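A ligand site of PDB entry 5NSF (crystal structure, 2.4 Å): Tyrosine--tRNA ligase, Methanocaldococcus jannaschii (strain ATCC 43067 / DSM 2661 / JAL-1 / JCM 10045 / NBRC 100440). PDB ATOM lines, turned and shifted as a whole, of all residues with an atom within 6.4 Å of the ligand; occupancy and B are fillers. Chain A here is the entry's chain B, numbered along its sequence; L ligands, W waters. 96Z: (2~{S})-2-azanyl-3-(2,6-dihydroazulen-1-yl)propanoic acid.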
ATOM      1  N   ILE A  45      25.182  18.896  24.501  1.00  0.00           N
ATOM      2  CA  ILE A  45      25.938  17.777  23.972  1.00  0.00           C
ATOM      3  C   ILE A  45      24.983  16.601  23.846  1.00  0.00           C
ATOM      4  O   ILE A  45      24.007  16.500  24.591  1.00  0.00           O
ATOM      5  CB  ILE A  45      27.148  17.408  24.865  1.00  0.00           C
ATOM      6  CG1 ILE A  45      27.997  16.307  24.210  1.00  0.00           C
ATOM      7  CG2 ILE A  45      26.675  16.948  26.245  1.00  0.00           C
ATOM      8  CD1 ILE A  45      29.371  16.149  24.817  1.00  0.00           C
ATOM      9  N   GLY A  46      25.260  15.719  22.890  1.00  0.00           N
ATOM     10  CA  GLY A  46      24.455  14.529  22.707  1.00  0.00           C
ATOM     11  C   GLY A  46      25.309  13.283  22.656  1.00  0.00           C
ATOM     12  O   GLY A  46      26.466  13.308  22.240  1.00  0.00           O
ATOM     13  N   PHE A  47      24.705  12.169  23.086  1.00  0.00           N
ATOM     14  CA  PHE A  47      25.372  10.876  23.106  1.00  0.00           C
ATOM     15  C   PHE A  47      24.415   9.805  22.602  1.00  0.00           C
ATOM     16  O   PHE A  47      23.282   9.724  23.072  1.00  0.00           O
ATOM     17  CB  PHE A  47      25.833  10.506  24.522  1.00  0.00           C
ATOM     18  CG  PHE A  47      26.758  11.498  25.143  1.00  0.00           C
ATOM     19  CD1 PHE A  47      28.108  11.511  24.814  1.00  0.00           C
ATOM     20  CD2 PHE A  47      26.292  12.409  26.076  1.00  0.00           C
ATOM     21  CE1 PHE A  47      28.965  12.421  25.405  1.00  0.00           C
ATOM     22  CE2 PHE A  47      27.151  13.323  26.654  1.00  0.00           C
ATOM     23  CZ  PHE A  47      28.480  13.329  26.316  1.00  0.00           C
ATOM     24  N   GLU A  48      24.885   8.980  21.671  1.00  0.00           N
ATOM     25  CA  GLU A  48      24.205   7.724  21.416  1.00  0.00           C
ATOM     26  C   GLU A  48      24.238   6.912  22.711  1.00  0.00           C
ATOM     27  O   GLU A  48      25.340   6.629  23.217  1.00  0.00           O
ATOM     28  CB  GLU A  48      24.867   6.940  20.297  1.00  0.00           C
ATOM     29  CG  GLU A  48      24.862   7.610  18.941  1.00  0.00           C
ATOM     30  CD  GLU A  48      25.467   6.707  17.873  1.00  0.00           C
ATOM     31  OE1 GLU A  48      25.348   5.477  18.008  1.00  0.00           O
ATOM     32  OE2 GLU A  48      26.054   7.240  16.916  1.00  0.00           O
ATOM     33  N   TRP A  77      21.341  15.676  25.179  1.00  0.00           N
ATOM     34  CA  TRP A  77      20.489  15.071  24.162  1.00  0.00           C
ATOM     35  C   TRP A  77      20.838  13.592  24.057  1.00  0.00           C
ATOM     36  O   TRP A  77      21.907  13.238  23.559  1.00  0.00           O
ATOM     37  CB  TRP A  77      20.678  15.799  22.833  1.00  0.00           C
ATOM     38  CG  TRP A  77      19.781  15.337  21.720  1.00  0.00           C
ATOM     39  CD1 TRP A  77      19.936  14.232  20.946  1.00  0.00           C
ATOM     40  CD2 TRP A  77      18.594  16.003  21.251  1.00  0.00           C
ATOM     41  NE1 TRP A  77      18.917  14.159  20.026  1.00  0.00           N
ATOM     42  CE2 TRP A  77      18.079  15.231  20.195  1.00  0.00           C
ATOM     43  CE3 TRP A  77      17.926  17.172  21.624  1.00  0.00           C
ATOM     44  CZ2 TRP A  77      16.924  15.591  19.504  1.00  0.00           C
ATOM     45  CZ3 TRP A  77      16.775  17.525  20.940  1.00  0.00           C
ATOM     46  CH2 TRP A  77      16.282  16.734  19.897  1.00  0.00           C
ATOM     47  N   ALA A  79      20.545  10.558  22.192  1.00  0.00           N
ATOM     48  CA  ALA A  79      20.191  10.325  20.793  1.00  0.00           C
ATOM     49  C   ALA A  79      19.863   8.846  20.588  1.00  0.00           C
ATOM     50  O   ALA A  79      20.614   8.079  19.981  1.00  0.00           O
ATOM     51  CB  ALA A  79      21.313  10.780  19.881  1.00  0.00           C
ATOM     52  N   LEU A  81      17.203   7.720  18.840  1.00  0.00           N
ATOM     53  CA  LEU A  81      16.867   7.543  17.435  1.00  0.00           C
ATOM     54  C   LEU A  81      18.128   7.592  16.566  1.00  0.00           C
ATOM     55  O   LEU A  81      18.227   6.867  15.573  1.00  0.00           O
ATOM     56  CB  LEU A  81      15.859   8.614  17.010  1.00  0.00           C
ATOM     57  CG  LEU A  81      15.235   8.525  15.611  1.00  0.00           C
ATOM     58  CD1 LEU A  81      14.730   7.122  15.325  1.00  0.00           C
ATOM     59  CD2 LEU A  81      14.091   9.523  15.521  1.00  0.00           C
ATOM     60  N   GLY A  82      19.081   8.458  16.924  1.00  0.00           N
ATOM     61  CA  GLY A  82      20.355   8.459  16.234  1.00  0.00           C
ATOM     62  C   GLY A  82      21.082   7.128  16.330  1.00  0.00           C
ATOM     63  O   GLY A  82      21.614   6.615  15.344  1.00  0.00           O
ATOM     64  N   ALA A  83      21.137   6.552  17.539  1.00  0.00           N
ATOM     65  CA  ALA A  83      21.746   5.245  17.710  1.00  0.00           C
ATOM     66  C   ALA A  83      21.033   4.183  16.887  1.00  0.00           C
ATOM     67  O   ALA A  83      21.665   3.238  16.396  1.00  0.00           O
ATOM     68  CB  ALA A  83      21.735   4.855  19.190  1.00  0.00           C
ATOM     69  N   LEU A  85      19.450   4.692  13.913  1.00  0.00           N
ATOM     70  CA  LEU A  85      19.906   4.874  12.542  1.00  0.00           C
ATOM     71  C   LEU A  85      21.332   4.394  12.356  1.00  0.00           C
ATOM     72  O   LEU A  85      21.748   4.123  11.217  1.00  0.00           O
ATOM     73  CB  LEU A  85      19.796   6.353  12.155  1.00  0.00           C
ATOM     74  CG  LEU A  85      18.387   6.942  12.108  1.00  0.00           C
ATOM     75  CD1 LEU A  85      18.460   8.457  11.952  1.00  0.00           C
ATOM     76  CD2 LEU A  85      17.580   6.344  10.973  1.00  0.00           C
ATOM     77  N   ASN A 121      12.267  14.231  18.128  1.00  0.00           N
ATOM     78  CA  ASN A 121      12.849  14.094  16.798  1.00  0.00           C
ATOM     79  C   ASN A 121      11.833  13.694  15.735  1.00  0.00           C
ATOM     80  O   ASN A 121      12.190  13.675  14.553  1.00  0.00           O
ATOM     81  CB  ASN A 121      13.946  13.034  16.816  1.00  0.00           C
ATOM     82  CG  ASN A 121      15.323  13.605  17.076  1.00  0.00           C
ATOM     83  OD1 ASN A 121      15.528  14.811  16.982  1.00  0.00           O
ATOM     84  ND2 ASN A 121      16.271  12.731  17.391  1.00  0.00           N
ATOM     85  N   TYR A 126       9.650  19.275  13.275  1.00  0.00           N
ATOM     86  CA  TYR A 126      11.045  18.838  13.320  1.00  0.00           C
ATOM     87  C   TYR A 126      11.402  18.034  12.086  1.00  0.00           C
ATOM     88  O   TYR A 126      12.424  18.273  11.442  1.00  0.00           O
ATOM     89  CB  TYR A 126      11.290  18.031  14.595  1.00  0.00           C
ATOM     90  CG  TYR A 126      12.748  17.679  14.848  1.00  0.00           C
ATOM     91  CD1 TYR A 126      13.387  16.709  14.095  1.00  0.00           C
ATOM     92  CD2 TYR A 126      13.468  18.326  15.843  1.00  0.00           C
ATOM     93  CE1 TYR A 126      14.713  16.386  14.329  1.00  0.00           C
ATOM     94  CE2 TYR A 126      14.799  18.011  16.081  1.00  0.00           C
ATOM     95  CZ  TYR A 126      15.412  17.039  15.313  1.00  0.00           C
ATOM     96  OH  TYR A 126      16.731  16.731  15.551  1.00  0.00           O
ATOM     97  N   ILE A 149      32.022   8.186  12.856  1.00  0.00           N
ATOM     98  CA  ILE A 149      30.892   7.879  13.713  1.00  0.00           C
ATOM     99  C   ILE A 149      30.150   6.633  13.262  1.00  0.00           C
ATOM    100  O   ILE A 149      29.710   5.829  14.091  1.00  0.00           O
ATOM    101  CB  ILE A 149      29.929   9.084  13.802  1.00  0.00           C
ATOM    102  CG1 ILE A 149      30.614  10.278  14.475  1.00  0.00           C
ATOM    103  CG2 ILE A 149      28.690   8.712  14.595  1.00  0.00           C
ATOM    104  CD1 ILE A 149      30.043  11.621  14.064  1.00  0.00           C
ATOM    105  N   TYR A 163      21.329  10.593   9.606  1.00  0.00           N
ATOM    106  CA  TYR A 163      21.858  10.839  10.941  1.00  0.00           C
ATOM    107  C   TYR A 163      22.480  12.217  11.105  1.00  0.00           C
ATOM    108  O   TYR A 163      22.064  12.957  12.009  1.00  0.00           O
ATOM    109  CB  TYR A 163      22.850   9.704  11.208  1.00  0.00           C
ATOM    110  CG  TYR A 163      23.536   9.681  12.549  1.00  0.00           C
ATOM    111  CD1 TYR A 163      24.511  10.621  12.885  1.00  0.00           C
ATOM    112  CD2 TYR A 163      23.276   8.672  13.458  1.00  0.00           C
ATOM    113  CE1 TYR A 163      25.161  10.569  14.099  1.00  0.00           C
ATOM    114  CE2 TYR A 163      23.917   8.604  14.664  1.00  0.00           C
ATOM    115  CZ  TYR A 163      24.858   9.557  14.990  1.00  0.00           C
ATOM    116  OH  TYR A 163      25.494   9.482  16.192  1.00  0.00           O
ATOM    117  N   PRO A 164      23.454  12.634  10.277  1.00  0.00           N
ATOM    118  CA  PRO A 164      24.092  13.942  10.534  1.00  0.00           C
ATOM    119  C   PRO A 164      23.154  15.137  10.410  1.00  0.00           C
ATOM    120  O   PRO A 164      23.250  16.068  11.215  1.00  0.00           O
ATOM    121  CB  PRO A 164      25.201  13.990   9.477  1.00  0.00           C
ATOM    122  CG  PRO A 164      24.770  13.034   8.403  1.00  0.00           C
ATOM    123  CD  PRO A 164      24.039  11.939   9.128  1.00  0.00           C
ATOM    124  N   MET A 166      20.034  15.145  11.088  1.00  0.00           N
ATOM    125  CA  MET A 166      19.243  15.150  12.329  1.00  0.00           C
ATOM    126  C   MET A 166      20.024  15.800  13.469  1.00  0.00           C
ATOM    127  O   MET A 166      19.438  16.521  14.290  1.00  0.00           O
ATOM    128  CB  MET A 166      18.857  13.718  12.707  1.00  0.00           C
ATOM    129  CG  MET A 166      18.004  12.979  11.702  1.00  0.00           C
ATOM    130  SD  MET A 166      16.936  11.747  12.454  1.00  0.00           S
ATOM    131  CE  MET A 166      15.752  12.753  13.329  1.00  0.00           C
ATOM    132  N   GLN A 167      21.335  15.561  13.531  1.00  0.00           N
ATOM    133  CA  GLN A 167      22.160  16.189  14.558  1.00  0.00           C
ATOM    134  C   GLN A 167      22.281  17.689  14.323  1.00  0.00           C
ATOM    135  O   GLN A 167      22.267  18.471  15.279  1.00  0.00           O
ATOM    136  CB  GLN A 167      23.534  15.532  14.579  1.00  0.00           C
ATOM    137  CG  GLN A 167      24.440  16.049  15.676  1.00  0.00           C
ATOM    138  CD  GLN A 167      25.671  15.175  15.870  1.00  0.00           C
ATOM    139  OE1 GLN A 167      25.715  14.038  15.421  1.00  0.00           O
ATOM    140  NE2 GLN A 167      26.678  15.710  16.556  1.00  0.00           N
ATOM    141  N   VAL A 168      22.382  18.116  13.062  1.00  0.00           N
ATOM    142  CA  VAL A 168      22.394  19.535  12.765  1.00  0.00           C
ATOM    143  C   VAL A 168      21.101  20.185  13.237  1.00  0.00           C
ATOM    144  O   VAL A 168      21.107  21.294  13.779  1.00  0.00           O
ATOM    145  CB  VAL A 168      22.615  19.756  11.255  1.00  0.00           C
ATOM    146  CG1 VAL A 168      22.310  21.203  10.866  1.00  0.00           C
ATOM    147  CG2 VAL A 168      24.042  19.386  10.878  1.00  0.00           C
ATOM    148  N   ALA A 170      18.972  19.201  15.667  1.00  0.00           N
ATOM    149  CA  ALA A 170      18.835  19.263  17.123  1.00  0.00           C
ATOM    150  C   ALA A 170      19.506  20.515  17.676  1.00  0.00           C
ATOM    151  O   ALA A 170      18.967  21.164  18.580  1.00  0.00           O
ATOM    152  CB  ALA A 170      19.418  18.003  17.761  1.00  0.00           C
ATOM    153  N   ILE A 171      20.669  20.870  17.137  1.00  0.00           N
ATOM    154  CA  ILE A 171      21.321  22.120  17.515  1.00  0.00           C
ATOM    155  C   ILE A 171      20.390  23.287  17.235  1.00  0.00           C
ATOM    156  O   ILE A 171      20.180  24.156  18.087  1.00  0.00           O
ATOM    157  CB  ILE A 171      22.655  22.259  16.758  1.00  0.00           C
ATOM    158  CG1 ILE A 171      23.667  21.232  17.270  1.00  0.00           C
ATOM    159  CG2 ILE A 171      23.198  23.683  16.883  1.00  0.00           C
ATOM    160  CD1 ILE A 171      24.902  21.080  16.399  1.00  0.00           C
ATOM    161  N   GLU A 184      35.548  13.868  16.916  1.00  0.00           N
ATOM    162  CA  GLU A 184      34.913  13.119  15.840  1.00  0.00           C
ATOM    163  C   GLU A 184      33.628  13.789  15.382  1.00  0.00           C
ATOM    164  O   GLU A 184      33.147  13.497  14.279  1.00  0.00           O
ATOM    165  CB  GLU A 184      34.644  11.673  16.278  1.00  0.00           C
ATOM    166  CG  GLU A 184      33.578  11.506  17.363  1.00  0.00           C
ATOM    167  CD  GLU A 184      34.087  11.813  18.754  1.00  0.00           C
ATOM    168  OE1 GLU A 184      35.319  11.819  18.965  1.00  0.00           O
ATOM    169  OE2 GLU A 184      33.249  12.052  19.647  1.00  0.00           O
ATOM    170  N   GLN A 185      33.061  14.673  16.189  1.00  0.00           N
ATOM    171  CA  GLN A 185      31.890  15.471  15.819  1.00  0.00           C
ATOM    172  C   GLN A 185      32.247  16.675  14.965  1.00  0.00           C
ATOM    173  O   GLN A 185      31.363  17.465  14.633  1.00  0.00           O
ATOM    174  CB  GLN A 185      31.159  15.944  17.077  1.00  0.00           C
ATOM    175  CG  GLN A 185      30.889  14.838  18.087  1.00  0.00           C
ATOM    176  CD  GLN A 185      30.035  13.748  17.491  1.00  0.00           C
ATOM    177  OE1 GLN A 185      29.131  14.030  16.721  1.00  0.00           O
ATOM    178  NE2 GLN A 185      30.329  12.496  17.842  1.00  0.00           N
ATOM    179  N   ILE A 188      30.351  17.173  11.315  1.00  0.00           N
ATOM    180  CA  ILE A 188      28.922  17.408  11.457  1.00  0.00           C
ATOM    181  C   ILE A 188      28.677  18.809  11.989  1.00  0.00           C
ATOM    182  O   ILE A 188      27.802  19.535  11.497  1.00  0.00           O
ATOM    183  CB  ILE A 188      28.273  16.336  12.363  1.00  0.00           C
ATOM    184  CG1 ILE A 188      28.241  14.987  11.641  1.00  0.00           C
ATOM    185  CG2 ILE A 188      26.858  16.778  12.785  1.00  0.00           C
ATOM    186  CD1 ILE A 188      27.665  13.847  12.462  1.00  0.00           C
HETATM  187  C11 96Z L   1      23.185  12.747  17.887  1.00  0.00           C
HETATM  188  C14 96Z L   1      20.702  12.982  16.103  1.00  0.00           C
HETATM  189  C1  96Z L   1      26.701  11.853  18.504  1.00  0.00           C
HETATM  190  C10 96Z L   1      22.627  14.051  18.188  1.00  0.00           C
HETATM  191  C12 96Z L   1      22.632  11.768  16.907  1.00  0.00           C
HETATM  192  C13 96Z L   1      21.545  11.944  16.164  1.00  0.00           C
HETATM  193  C15 96Z L   1      20.625  14.172  16.718  1.00  0.00           C
HETATM  194  C16 96Z L   1      21.434  14.710  17.639  1.00  0.00           C
HETATM  195  C3  96Z L   1      27.622  10.749  18.974  1.00  0.00           C
HETATM  196  C6  96Z L   1      25.257  11.439  18.749  1.00  0.00           C
HETATM  197  C7  96Z L   1      24.318  12.630  18.685  1.00  0.00           C
HETATM  198  C8  96Z L   1      24.444  13.797  19.445  1.00  0.00           C
HETATM  199  C9  96Z L   1      23.404  14.683  19.144  1.00  0.00           C
HETATM  200  N17 96Z L   1      26.906  12.087  17.065  1.00  0.00           N
HETATM  201  O4  96Z L   1      27.338  10.153  20.062  1.00  0.00           O
HETATM  202  O5  96Z L   1      28.653  10.523  18.299  1.00  0.00           O
HETATM  203  O   HOH W   1      22.950  18.001  18.226  1.00  0.00           O
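Residues that only touch the ligand: Gly 46 (3.3 Å), Ala 79 (3.4 Å), Trp 77 (3.5 Å), Met 166 (3.6 Å), Gly 82 (3.7 Å), Phe 47 (3.7 Å) and Ala 170 (3.9 Å).
Hydrophobic or aromatic side chains within 4 Å of the ligand: Trp 77, Ala 79, Tyr 163, Met 166 and Ala 170.
Within 4 Å of the ligand: Gly 46, Phe 47, Glu 48, Trp 77, Ala 79, Gly 82, Tyr 163, Met 166, Gln 167, Ala 170 and Gln 185.
The side-chain hydroxyl (OH) of Tyr 126 lies within hydrogen-bond range of the backbone NH (N) of Ala 170 (3.3 Å).
NE2 of Gln 167 sits at hydrogen-bond distance from OE1 of Gln 185, at 3.0 Å.
NE2 of Gln 185 sits close to OE2 of Glu 184 (3.5 Å).
The backbone NH (N) of Trp 77 sits at hydrogen-bond distance from the backbone carbonyl oxygen (O) of Ile 45 (2.9 Å).
OH of Tyr 163 lies within hydrogen-bond range of OE2 of Glu 48, 2.4 Å away.
The backbone carbonyl oxygen (O) of Phe 47 lies within hydrogen-bond range of the backbone NH (N) of Ala 79, 3.0 Å away.
The backbone carbonyl oxygen of Trp 77 is in hydrogen-bond range of the backbone NH of Phe 47 (3.0 Å).
The backbone carbonyl oxygen (O) of Met 166 sits at hydrogen-bond distance from the side-chain hydroxyl (OH) of Tyr 126, 3.0 Å away.
OE1 of Gln 167 sits at hydrogen-bond distance from N17 of the ligand, at 2.8 Å.
The side-chain amide nitrogen of Gln 185 lies within hydrogen-bond range of an oxygen (O5) of the ligand (2.6 Å).
An oxygen (O4) of the ligand is in hydrogen-bond range of the backbone NH of Glu 48, 3.2 Å away.
The side-chain hydroxyl of Tyr 163 lies within hydrogen-bond range of a nitrogen (N17) of the ligand, at 3.1 Å.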
